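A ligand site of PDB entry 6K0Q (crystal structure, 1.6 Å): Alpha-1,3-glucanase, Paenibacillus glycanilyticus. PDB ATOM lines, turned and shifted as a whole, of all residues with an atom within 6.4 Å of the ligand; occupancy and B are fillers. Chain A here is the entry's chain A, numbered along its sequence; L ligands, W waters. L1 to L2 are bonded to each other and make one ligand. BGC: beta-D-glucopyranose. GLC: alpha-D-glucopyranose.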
ATOM      1  N   THR A  86      -2.642 -24.973 -24.598  1.00  0.00           N
ATOM      2  CA  THR A  86      -1.680 -23.980 -24.153  1.00  0.00           C
ATOM      3  C   THR A  86      -2.451 -22.708 -23.833  1.00  0.00           C
ATOM      4  O   THR A  86      -3.537 -22.468 -24.373  1.00  0.00           O
ATOM      5  CB  THR A  86      -0.622 -23.662 -25.210  1.00  0.00           C
ATOM      6  OG1 THR A  86      -1.243 -22.992 -26.326  1.00  0.00           O
ATOM      7  CG2 THR A  86       0.071 -24.927 -25.696  1.00  0.00           C
ATOM      8  N   PHE A 101       2.019 -16.426 -16.830  1.00  0.00           N
ATOM      9  CA  PHE A 101       2.701 -17.697 -17.063  1.00  0.00           C
ATOM     10  C   PHE A 101       2.232 -18.314 -18.369  1.00  0.00           C
ATOM     11  O   PHE A 101       1.038 -18.279 -18.678  1.00  0.00           O
ATOM     12  CB  PHE A 101       2.371 -18.689 -15.949  1.00  0.00           C
ATOM     13  CG  PHE A 101       3.060 -18.412 -14.653  1.00  0.00           C
ATOM     14  CD1 PHE A 101       4.320 -18.923 -14.395  1.00  0.00           C
ATOM     15  CD2 PHE A 101       2.420 -17.671 -13.676  1.00  0.00           C
ATOM     16  CE1 PHE A 101       4.949 -18.677 -13.183  1.00  0.00           C
ATOM     17  CE2 PHE A 101       3.044 -17.433 -12.453  1.00  0.00           C
ATOM     18  CZ  PHE A 101       4.300 -17.941 -12.204  1.00  0.00           C
ATOM     19  N   ASN A 102       3.158 -18.942 -19.098  1.00  0.00           N
ATOM     20  CA  ASN A 102       2.837 -19.763 -20.258  1.00  0.00           C
ATOM     21  C   ASN A 102       2.615 -21.190 -19.738  1.00  0.00           C
ATOM     22  O   ASN A 102       3.568 -21.893 -19.400  1.00  0.00           O
ATOM     23  CB  ASN A 102       3.961 -19.699 -21.290  1.00  0.00           C
ATOM     24  CG  ASN A 102       3.674 -20.513 -22.537  1.00  0.00           C
ATOM     25  OD1 ASN A 102       3.014 -21.545 -22.503  1.00  0.00           O
ATOM     26  ND2 ASN A 102       4.206 -20.049 -23.667  1.00  0.00           N
ATOM     27  N   VAL A 103       1.345 -21.605 -19.655  1.00  0.00           N
ATOM     28  CA  VAL A 103       0.997 -22.920 -19.126  1.00  0.00           C
ATOM     29  C   VAL A 103       0.622 -23.814 -20.294  1.00  0.00           C
ATOM     30  O   VAL A 103       0.069 -23.371 -21.305  1.00  0.00           O
ATOM     31  CB  VAL A 103      -0.140 -22.841 -18.077  1.00  0.00           C
ATOM     32  CG1 VAL A 103       0.353 -22.079 -16.854  1.00  0.00           C
ATOM     33  CG2 VAL A 103      -1.392 -22.195 -18.666  1.00  0.00           C
ATOM     34  N   SER A 104       0.947 -25.105 -20.156  1.00  0.00           N
ATOM     35  CA  SER A 104       0.799 -26.020 -21.282  1.00  0.00           C
ATOM     36  C   SER A 104       0.754 -27.453 -20.787  1.00  0.00           C
ATOM     37  O   SER A 104       1.421 -27.805 -19.820  1.00  0.00           O
ATOM     38  CB  SER A 104       1.961 -25.862 -22.263  1.00  0.00           C
ATOM     39  OG  SER A 104       1.815 -26.795 -23.318  1.00  0.00           O
ATOM     40  N   LYS A 106       1.752 -29.740 -23.057  1.00  0.00           N
ATOM     41  CA  LYS A 106       2.588 -30.386 -24.074  1.00  0.00           C
ATOM     42  C   LYS A 106       3.322 -31.601 -23.514  1.00  0.00           C
ATOM     43  O   LYS A 106       3.428 -32.643 -24.186  1.00  0.00           O
ATOM     44  CB  LYS A 106       3.596 -29.378 -24.640  1.00  0.00           C
ATOM     45  CG  LYS A 106       4.521 -29.987 -25.692  1.00  0.00           C
ATOM     46  CD  LYS A 106       5.589 -29.006 -26.123  1.00  0.00           C
ATOM     47  CE  LYS A 106       6.511 -29.678 -27.146  1.00  0.00           C
ATOM     48  NZ  LYS A 106       7.365 -28.703 -27.847  1.00  0.00           N
ATOM     49  N   PHE A 107       3.827 -31.498 -22.288  1.00  0.00           N
ATOM     50  CA  PHE A 107       4.681 -32.541 -21.732  1.00  0.00           C
ATOM     51  C   PHE A 107       3.978 -33.430 -20.716  1.00  0.00           C
ATOM     52  O   PHE A 107       4.601 -34.394 -20.228  1.00  0.00           O
ATOM     53  CB  PHE A 107       5.922 -31.910 -21.095  1.00  0.00           C
ATOM     54  CG  PHE A 107       6.844 -31.296 -22.106  1.00  0.00           C
ATOM     55  CD1 PHE A 107       7.654 -32.105 -22.890  1.00  0.00           C
ATOM     56  CD2 PHE A 107       6.869 -29.922 -22.323  1.00  0.00           C
ATOM     57  CE1 PHE A 107       8.514 -31.562 -23.839  1.00  0.00           C
ATOM     58  CE2 PHE A 107       7.720 -29.362 -23.266  1.00  0.00           C
ATOM     59  CZ  PHE A 107       8.545 -30.186 -24.025  1.00  0.00           C
ATOM     60  N   ASP A 138       4.947 -27.730 -15.512  1.00  0.00           N
ATOM     61  CA  ASP A 138       5.506 -26.525 -14.898  1.00  0.00           C
ATOM     62  C   ASP A 138       5.545 -25.359 -15.871  1.00  0.00           C
ATOM     63  O   ASP A 138       5.795 -25.530 -17.069  1.00  0.00           O
ATOM     64  CB  ASP A 138       6.943 -26.747 -14.397  1.00  0.00           C
ATOM     65  CG  ASP A 138       7.048 -27.734 -13.250  1.00  0.00           C
ATOM     66  OD1 ASP A 138       6.018 -28.174 -12.715  1.00  0.00           O
ATOM     67  OD2 ASP A 138       8.200 -28.031 -12.889  1.00  0.00           O
ATOM     68  N   ALA A 139       5.380 -24.150 -15.323  1.00  0.00           N
ATOM     69  CA  ALA A 139       5.561 -22.925 -16.094  1.00  0.00           C
ATOM     70  C   ALA A 139       6.568 -22.056 -15.368  1.00  0.00           C
ATOM     71  O   ALA A 139       6.480 -21.869 -14.151  1.00  0.00           O
ATOM     72  CB  ALA A 139       4.232 -22.173 -16.268  1.00  0.00           C
ATOM     73  N   GLN A 140       7.536 -21.512 -16.106  1.00  0.00           N
ATOM     74  CA  GLN A 140       8.624 -20.720 -15.549  1.00  0.00           C
ATOM     75  C   GLN A 140       8.459 -19.271 -15.972  1.00  0.00           C
ATOM     76  O   GLN A 140       8.178 -18.980 -17.144  1.00  0.00           O
ATOM     77  CB  GLN A 140       9.984 -21.243 -16.033  1.00  0.00           C
ATOM     78  CG  GLN A 140      10.279 -22.711 -15.718  1.00  0.00           C
ATOM     79  CD  GLN A 140       9.521 -23.678 -16.616  1.00  0.00           C
ATOM     80  OE1 GLN A 140       9.212 -23.379 -17.786  1.00  0.00           O
ATOM     81  NE2 GLN A 140       9.205 -24.848 -16.077  1.00  0.00           N
ATOM     82  N   LEU A 141       8.657 -18.348 -15.027  1.00  0.00           N
ATOM     83  CA  LEU A 141       8.487 -16.926 -15.335  1.00  0.00           C
ATOM     84  C   LEU A 141       9.417 -16.063 -14.493  1.00  0.00           C
ATOM     85  O   LEU A 141       9.514 -16.253 -13.272  1.00  0.00           O
ATOM     86  CB  LEU A 141       7.038 -16.509 -15.105  1.00  0.00           C
ATOM     87  CG  LEU A 141       6.679 -15.085 -15.505  1.00  0.00           C
ATOM     88  CD1 LEU A 141       6.653 -15.001 -17.008  1.00  0.00           C
ATOM     89  CD2 LEU A 141       5.315 -14.737 -14.930  1.00  0.00           C
ATOM     90  N   MET A 142      10.127 -15.141 -15.131  1.00  0.00           N
ATOM     91  CA  MET A 142      10.920 -14.135 -14.445  1.00  0.00           C
ATOM     92  C   MET A 142      10.252 -12.777 -14.591  1.00  0.00           C
ATOM     93  O   MET A 142       9.740 -12.443 -15.665  1.00  0.00           O
ATOM     94  CB  MET A 142      12.355 -14.106 -15.000  1.00  0.00           C
ATOM     95  CG  MET A 142      13.312 -13.187 -14.253  1.00  0.00           C
ATOM     96  SD  MET A 142      15.057 -13.544 -14.602  1.00  0.00           S
ATOM     97  CE  MET A 142      15.400 -14.829 -13.429  1.00  0.00           C
ATOM     98  N   GLU A 218      18.604 -18.711 -25.770  1.00  0.00           N
ATOM     99  CA  GLU A 218      18.151 -20.037 -26.147  1.00  0.00           C
ATOM    100  C   GLU A 218      19.024 -20.532 -27.273  1.00  0.00           C
ATOM    101  O   GLU A 218      19.158 -19.870 -28.304  1.00  0.00           O
ATOM    102  CB  GLU A 218      16.687 -20.038 -26.581  1.00  0.00           C
ATOM    103  CG  GLU A 218      15.699 -19.634 -25.521  1.00  0.00           C
ATOM    104  CD  GLU A 218      14.267 -19.764 -26.010  1.00  0.00           C
ATOM    105  OE1 GLU A 218      14.043 -20.477 -27.026  1.00  0.00           O
ATOM    106  OE2 GLU A 218      13.381 -19.164 -25.390  1.00  0.00           O
ATOM    107  N   TRP A 240      18.798 -20.042 -15.135  1.00  0.00           N
ATOM    108  CA  TRP A 240      17.665 -19.247 -15.591  1.00  0.00           C
ATOM    109  C   TRP A 240      17.964 -18.479 -16.867  1.00  0.00           C
ATOM    110  O   TRP A 240      17.031 -17.928 -17.468  1.00  0.00           O
ATOM    111  CB  TRP A 240      17.240 -18.250 -14.502  1.00  0.00           C
ATOM    112  CG  TRP A 240      16.270 -18.811 -13.505  1.00  0.00           C
ATOM    113  CD1 TRP A 240      16.579 -19.390 -12.303  1.00  0.00           C
ATOM    114  CD2 TRP A 240      14.836 -18.855 -13.610  1.00  0.00           C
ATOM    115  NE1 TRP A 240      15.426 -19.784 -11.657  1.00  0.00           N
ATOM    116  CE2 TRP A 240      14.345 -19.464 -12.432  1.00  0.00           C
ATOM    117  CE3 TRP A 240      13.926 -18.442 -14.592  1.00  0.00           C
ATOM    118  CZ2 TRP A 240      12.985 -19.677 -12.201  1.00  0.00           C
ATOM    119  CZ3 TRP A 240      12.561 -18.646 -14.357  1.00  0.00           C
ATOM    120  CH2 TRP A 240      12.110 -19.261 -13.173  1.00  0.00           C
ATOM    121  N   LYS A 243      19.927 -21.347 -21.818  1.00  0.00           N
ATOM    122  CA  LYS A 243      18.987 -22.438 -22.065  1.00  0.00           C
ATOM    123  C   LYS A 243      19.401 -23.187 -23.320  1.00  0.00           C
ATOM    124  O   LYS A 243      19.379 -22.627 -24.415  1.00  0.00           O
ATOM    125  CB  LYS A 243      17.564 -21.893 -22.209  1.00  0.00           C
ATOM    126  CG  LYS A 243      17.085 -21.057 -21.007  1.00  0.00           C
ATOM    127  CD  LYS A 243      15.700 -20.485 -21.279  1.00  0.00           C
ATOM    128  CE  LYS A 243      15.283 -19.499 -20.185  1.00  0.00           C
ATOM    129  NZ  LYS A 243      13.909 -18.998 -20.446  1.00  0.00           N
ATOM    130  N   VAL A 245      18.226 -25.855 -25.859  1.00  0.00           N
ATOM    131  CA  VAL A 245      16.853 -26.206 -26.214  1.00  0.00           C
ATOM    132  C   VAL A 245      16.870 -27.247 -27.324  1.00  0.00           C
ATOM    133  O   VAL A 245      17.370 -26.971 -28.420  1.00  0.00           O
ATOM    134  CB  VAL A 245      16.037 -24.972 -26.608  1.00  0.00           C
ATOM    135  CG1 VAL A 245      14.583 -25.348 -26.862  1.00  0.00           C
ATOM    136  CG2 VAL A 245      16.124 -23.892 -25.517  1.00  0.00           C
ATOM    137  N   GLN A 248      11.908 -27.867 -30.530  1.00  0.00           N
ATOM    138  CA  GLN A 248      10.648 -28.114 -29.852  1.00  0.00           C
ATOM    139  C   GLN A 248       9.525 -28.510 -30.805  1.00  0.00           C
ATOM    140  O   GLN A 248       8.494 -28.994 -30.335  1.00  0.00           O
ATOM    141  CB  GLN A 248      10.238 -26.888 -29.021  1.00  0.00           C
ATOM    142  CG  GLN A 248      11.106 -26.705 -27.771  1.00  0.00           C
ATOM    143  CD  GLN A 248      11.019 -27.899 -26.819  1.00  0.00           C
ATOM    144  OE1 GLN A 248       9.940 -28.352 -26.477  1.00  0.00           O
ATOM    145  NE2 GLN A 248      12.171 -28.400 -26.377  1.00  0.00           N
ATOM    146  N   TRP A 274      16.580 -28.025 -21.958  1.00  0.00           N
ATOM    147  CA  TRP A 274      15.143 -28.192 -22.147  1.00  0.00           C
ATOM    148  C   TRP A 274      14.925 -29.189 -23.278  1.00  0.00           C
ATOM    149  O   TRP A 274      15.009 -28.830 -24.450  1.00  0.00           O
ATOM    150  CB  TRP A 274      14.493 -26.836 -22.431  1.00  0.00           C
ATOM    151  CG  TRP A 274      14.618 -25.963 -21.208  1.00  0.00           C
ATOM    152  CD1 TRP A 274      15.643 -25.105 -20.906  1.00  0.00           C
ATOM    153  CD2 TRP A 274      13.730 -25.931 -20.088  1.00  0.00           C
ATOM    154  NE1 TRP A 274      15.418 -24.521 -19.685  1.00  0.00           N
ATOM    155  CE2 TRP A 274      14.249 -25.013 -19.166  1.00  0.00           C
ATOM    156  CE3 TRP A 274      12.511 -26.565 -19.802  1.00  0.00           C
ATOM    157  CZ2 TRP A 274      13.622 -24.730 -17.953  1.00  0.00           C
ATOM    158  CZ3 TRP A 274      11.891 -26.292 -18.584  1.00  0.00           C
ATOM    159  CH2 TRP A 274      12.437 -25.371 -17.693  1.00  0.00           C
ATOM    160  N   GLY A 275      14.679 -30.446 -22.927  1.00  0.00           N
ATOM    161  CA  GLY A 275      14.528 -31.482 -23.917  1.00  0.00           C
ATOM    162  C   GLY A 275      13.181 -31.435 -24.603  1.00  0.00           C
ATOM    163  O   GLY A 275      12.306 -30.626 -24.310  1.00  0.00           O
ATOM    164  N   HIS A 305      12.599 -32.803 -19.280  1.00  0.00           N
ATOM    165  CA  HIS A 305      12.042 -33.382 -20.501  1.00  0.00           C
ATOM    166  C   HIS A 305      13.095 -34.144 -21.299  1.00  0.00           C
ATOM    167  O   HIS A 305      13.125 -34.109 -22.539  1.00  0.00           O
ATOM    168  CB  HIS A 305      11.347 -32.315 -21.341  1.00  0.00           C
ATOM    169  CG  HIS A 305      10.328 -31.538 -20.564  1.00  0.00           C
ATOM    170  ND1 HIS A 305      10.136 -30.180 -20.725  1.00  0.00           N
ATOM    171  CD2 HIS A 305       9.461 -31.931 -19.608  1.00  0.00           C
ATOM    172  CE1 HIS A 305       9.192 -29.776 -19.890  1.00  0.00           C
ATOM    173  NE2 HIS A 305       8.769 -30.813 -19.201  1.00  0.00           N
HETATM  174  C2  BGC L   1      10.180 -21.579 -23.447  1.00  0.00           C
HETATM  175  C3  BGC L   1       8.724 -21.274 -23.078  1.00  0.00           C
HETATM  176  C4  BGC L   1       8.646 -20.587 -21.723  1.00  0.00           C
HETATM  177  C5  BGC L   1       9.572 -19.371 -21.726  1.00  0.00           C
HETATM  178  C6  BGC L   1       9.447 -18.556 -20.444  1.00  0.00           C
HETATM  179  C1  BGC L   1      11.108 -20.388 -23.195  1.00  0.00           C
HETATM  180  O1  BGC L   1      12.457 -20.839 -23.274  1.00  0.00           O
HETATM  181  O2  BGC L   1      10.241 -21.916 -24.821  1.00  0.00           O
HETATM  182  O3  BGC L   1       7.973 -22.471 -23.049  1.00  0.00           O
HETATM  183  O4  BGC L   1       7.321 -20.182 -21.456  1.00  0.00           O
HETATM  184  O5  BGC L   1      10.890 -19.845 -21.898  1.00  0.00           O
HETATM  185  O6  BGC L   1       9.872 -19.343 -19.347  1.00  0.00           O
HETATM  186  C1  GLC L   2       6.986 -22.620 -23.994  1.00  0.00           C
HETATM  187  C2  GLC L   2       6.059 -23.765 -23.601  1.00  0.00           C
HETATM  188  C3  GLC L   2       6.719 -25.113 -23.876  1.00  0.00           C
HETATM  189  C4  GLC L   2       7.197 -25.165 -25.328  1.00  0.00           C
HETATM  190  C5  GLC L   2       8.051 -23.932 -25.650  1.00  0.00           C
HETATM  191  C6  GLC L   2       8.440 -23.947 -27.125  1.00  0.00           C
HETATM  192  O2  GLC L   2       5.702 -23.650 -22.234  1.00  0.00           O
HETATM  193  O3  GLC L   2       5.777 -26.149 -23.671  1.00  0.00           O
HETATM  194  O4  GLC L   2       7.955 -26.331 -25.575  1.00  0.00           O
HETATM  195  O5  GLC L   2       7.334 -22.740 -25.358  1.00  0.00           O
HETATM  196  O6  GLC L   2       7.268 -23.917 -27.925  1.00  0.00           O
HETATM  197  O   HOH W   1      12.897 -23.190 -22.196  1.00  0.00           O
HETATM  198  O   HOH W   2       6.621 -18.160 -22.833  1.00  0.00           O
HETATM  199  O   HOH W   3       6.714 -16.658 -20.680  1.00  0.00           O
HETATM  200  O   HOH W   4       4.754 -24.542 -19.528  1.00  0.00           O
HETATM  201  O   HOH W   5       3.344 -22.885 -24.722  1.00  0.00           O
HETATM  202  O   HOH W   6       7.799 -21.192 -28.984  1.00  0.00           O
HETATM  203  O   HOH W   7       3.580 -25.656 -25.090  1.00  0.00           O
HETATM  204  O   HOH W   8      10.283 -26.460 -23.756  1.00  0.00           O
HETATM  205  O   HOH W   9       6.300 -26.110 -28.808  1.00  0.00           O
HETATM  206  O   HOH W  10       6.479 -21.504 -19.024  1.00  0.00           O
HETATM  207  O   HOH W  11       9.141 -20.134 -26.707  1.00  0.00           O
HETATM  208  O   HOH W  12      12.311 -24.520 -24.362  1.00  0.00           O
HETATM  209  O   HOH W  13       7.683 -23.848 -20.027  1.00  0.00           O
HETATM  210  O   HOH W  14       5.032 -20.876 -26.366  1.00  0.00           O
HETATM  211  O   HOH W  15      13.809 -17.771 -23.115  1.00  0.00           O
HETATM  212  O   HOH W  16      12.301 -22.613 -26.377  1.00  0.00           O
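NZ of Lys 106 sits at hydrogen-bond distance from O of Gln 248 (2.7 Å).
O of Trp 274 sits at hydrogen-bond distance from NE2 of Gln 248, at 3.5 Å.
The backbone carbonyl oxygen (O) of Gly 275 sits at hydrogen-bond distance from the side-chain amide nitrogen (NE2) of Gln 248 (3.0 Å).
The backbone NH (N) of Lys 106 is in hydrogen-bond range of the side-chain hydroxyl (OG) of Ser 104, 3.0 Å away.
Residues that only touch the ligand: Phe 107 (3.8 Å).
Seven residues have an atom within 4 Å of the ligand: Asn 102, Lys 106, Phe 107, Gln 140, Glu 218, Lys 243 and Gln 248.
Along chain A the residues within 4 Å of the ligand span positions 102 to 248.
Water W2 lies within hydrogen-bond range of O4 of BGC L1 (2.5 Å) and ND2 of Asn 102 (3.2 Å).
Water W7 lies within hydrogen-bond range of O3 of GLC L2 (2.7 Å) and OG of Ser 104 (2.7 Å).
Water W10 lies within hydrogen-bond range of O4 of BGC L1, O of Asn 102 and N of Gln 140.
Water W8 bridges an oxygen (O4) of GLC L2 (3.0 Å) and the side-chain amide oxygen (OE1) of Gln 248 (3.3 Å).
Water W13 bridges the side-chain amide oxygen of Gln 140 (2.8 Å) and an oxygen (O2) of GLC L2 (3.0 Å).
Water W4 lies within hydrogen-bond range of the backbone carbonyl oxygen of Asp 138, the backbone carbonyl oxygen of Asn 102 and an oxygen (O2) of GLC L2.
O6 of BGC L1 lies within hydrogen-bond range of O of Gln 140 (2.8 Å).
OE2 of Glu 218 is in hydrogen-bond range of O1 of BGC L1, at 2.9 Å.
OE1 of Gln 248 sits at hydrogen-bond distance from O4 of GLC L2, 3.0 Å away.
NZ of Lys 106 lies within hydrogen-bond range of O4 of GLC L2, at 3.3 Å.
The side-chain amide oxygen (OD1) of Asn 102 is in hydrogen-bond range of an oxygen (O2) of GLC L2 (3.4 Å).
NZ of Lys 243 sits at hydrogen-bond distance from O5 of BGC L1.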
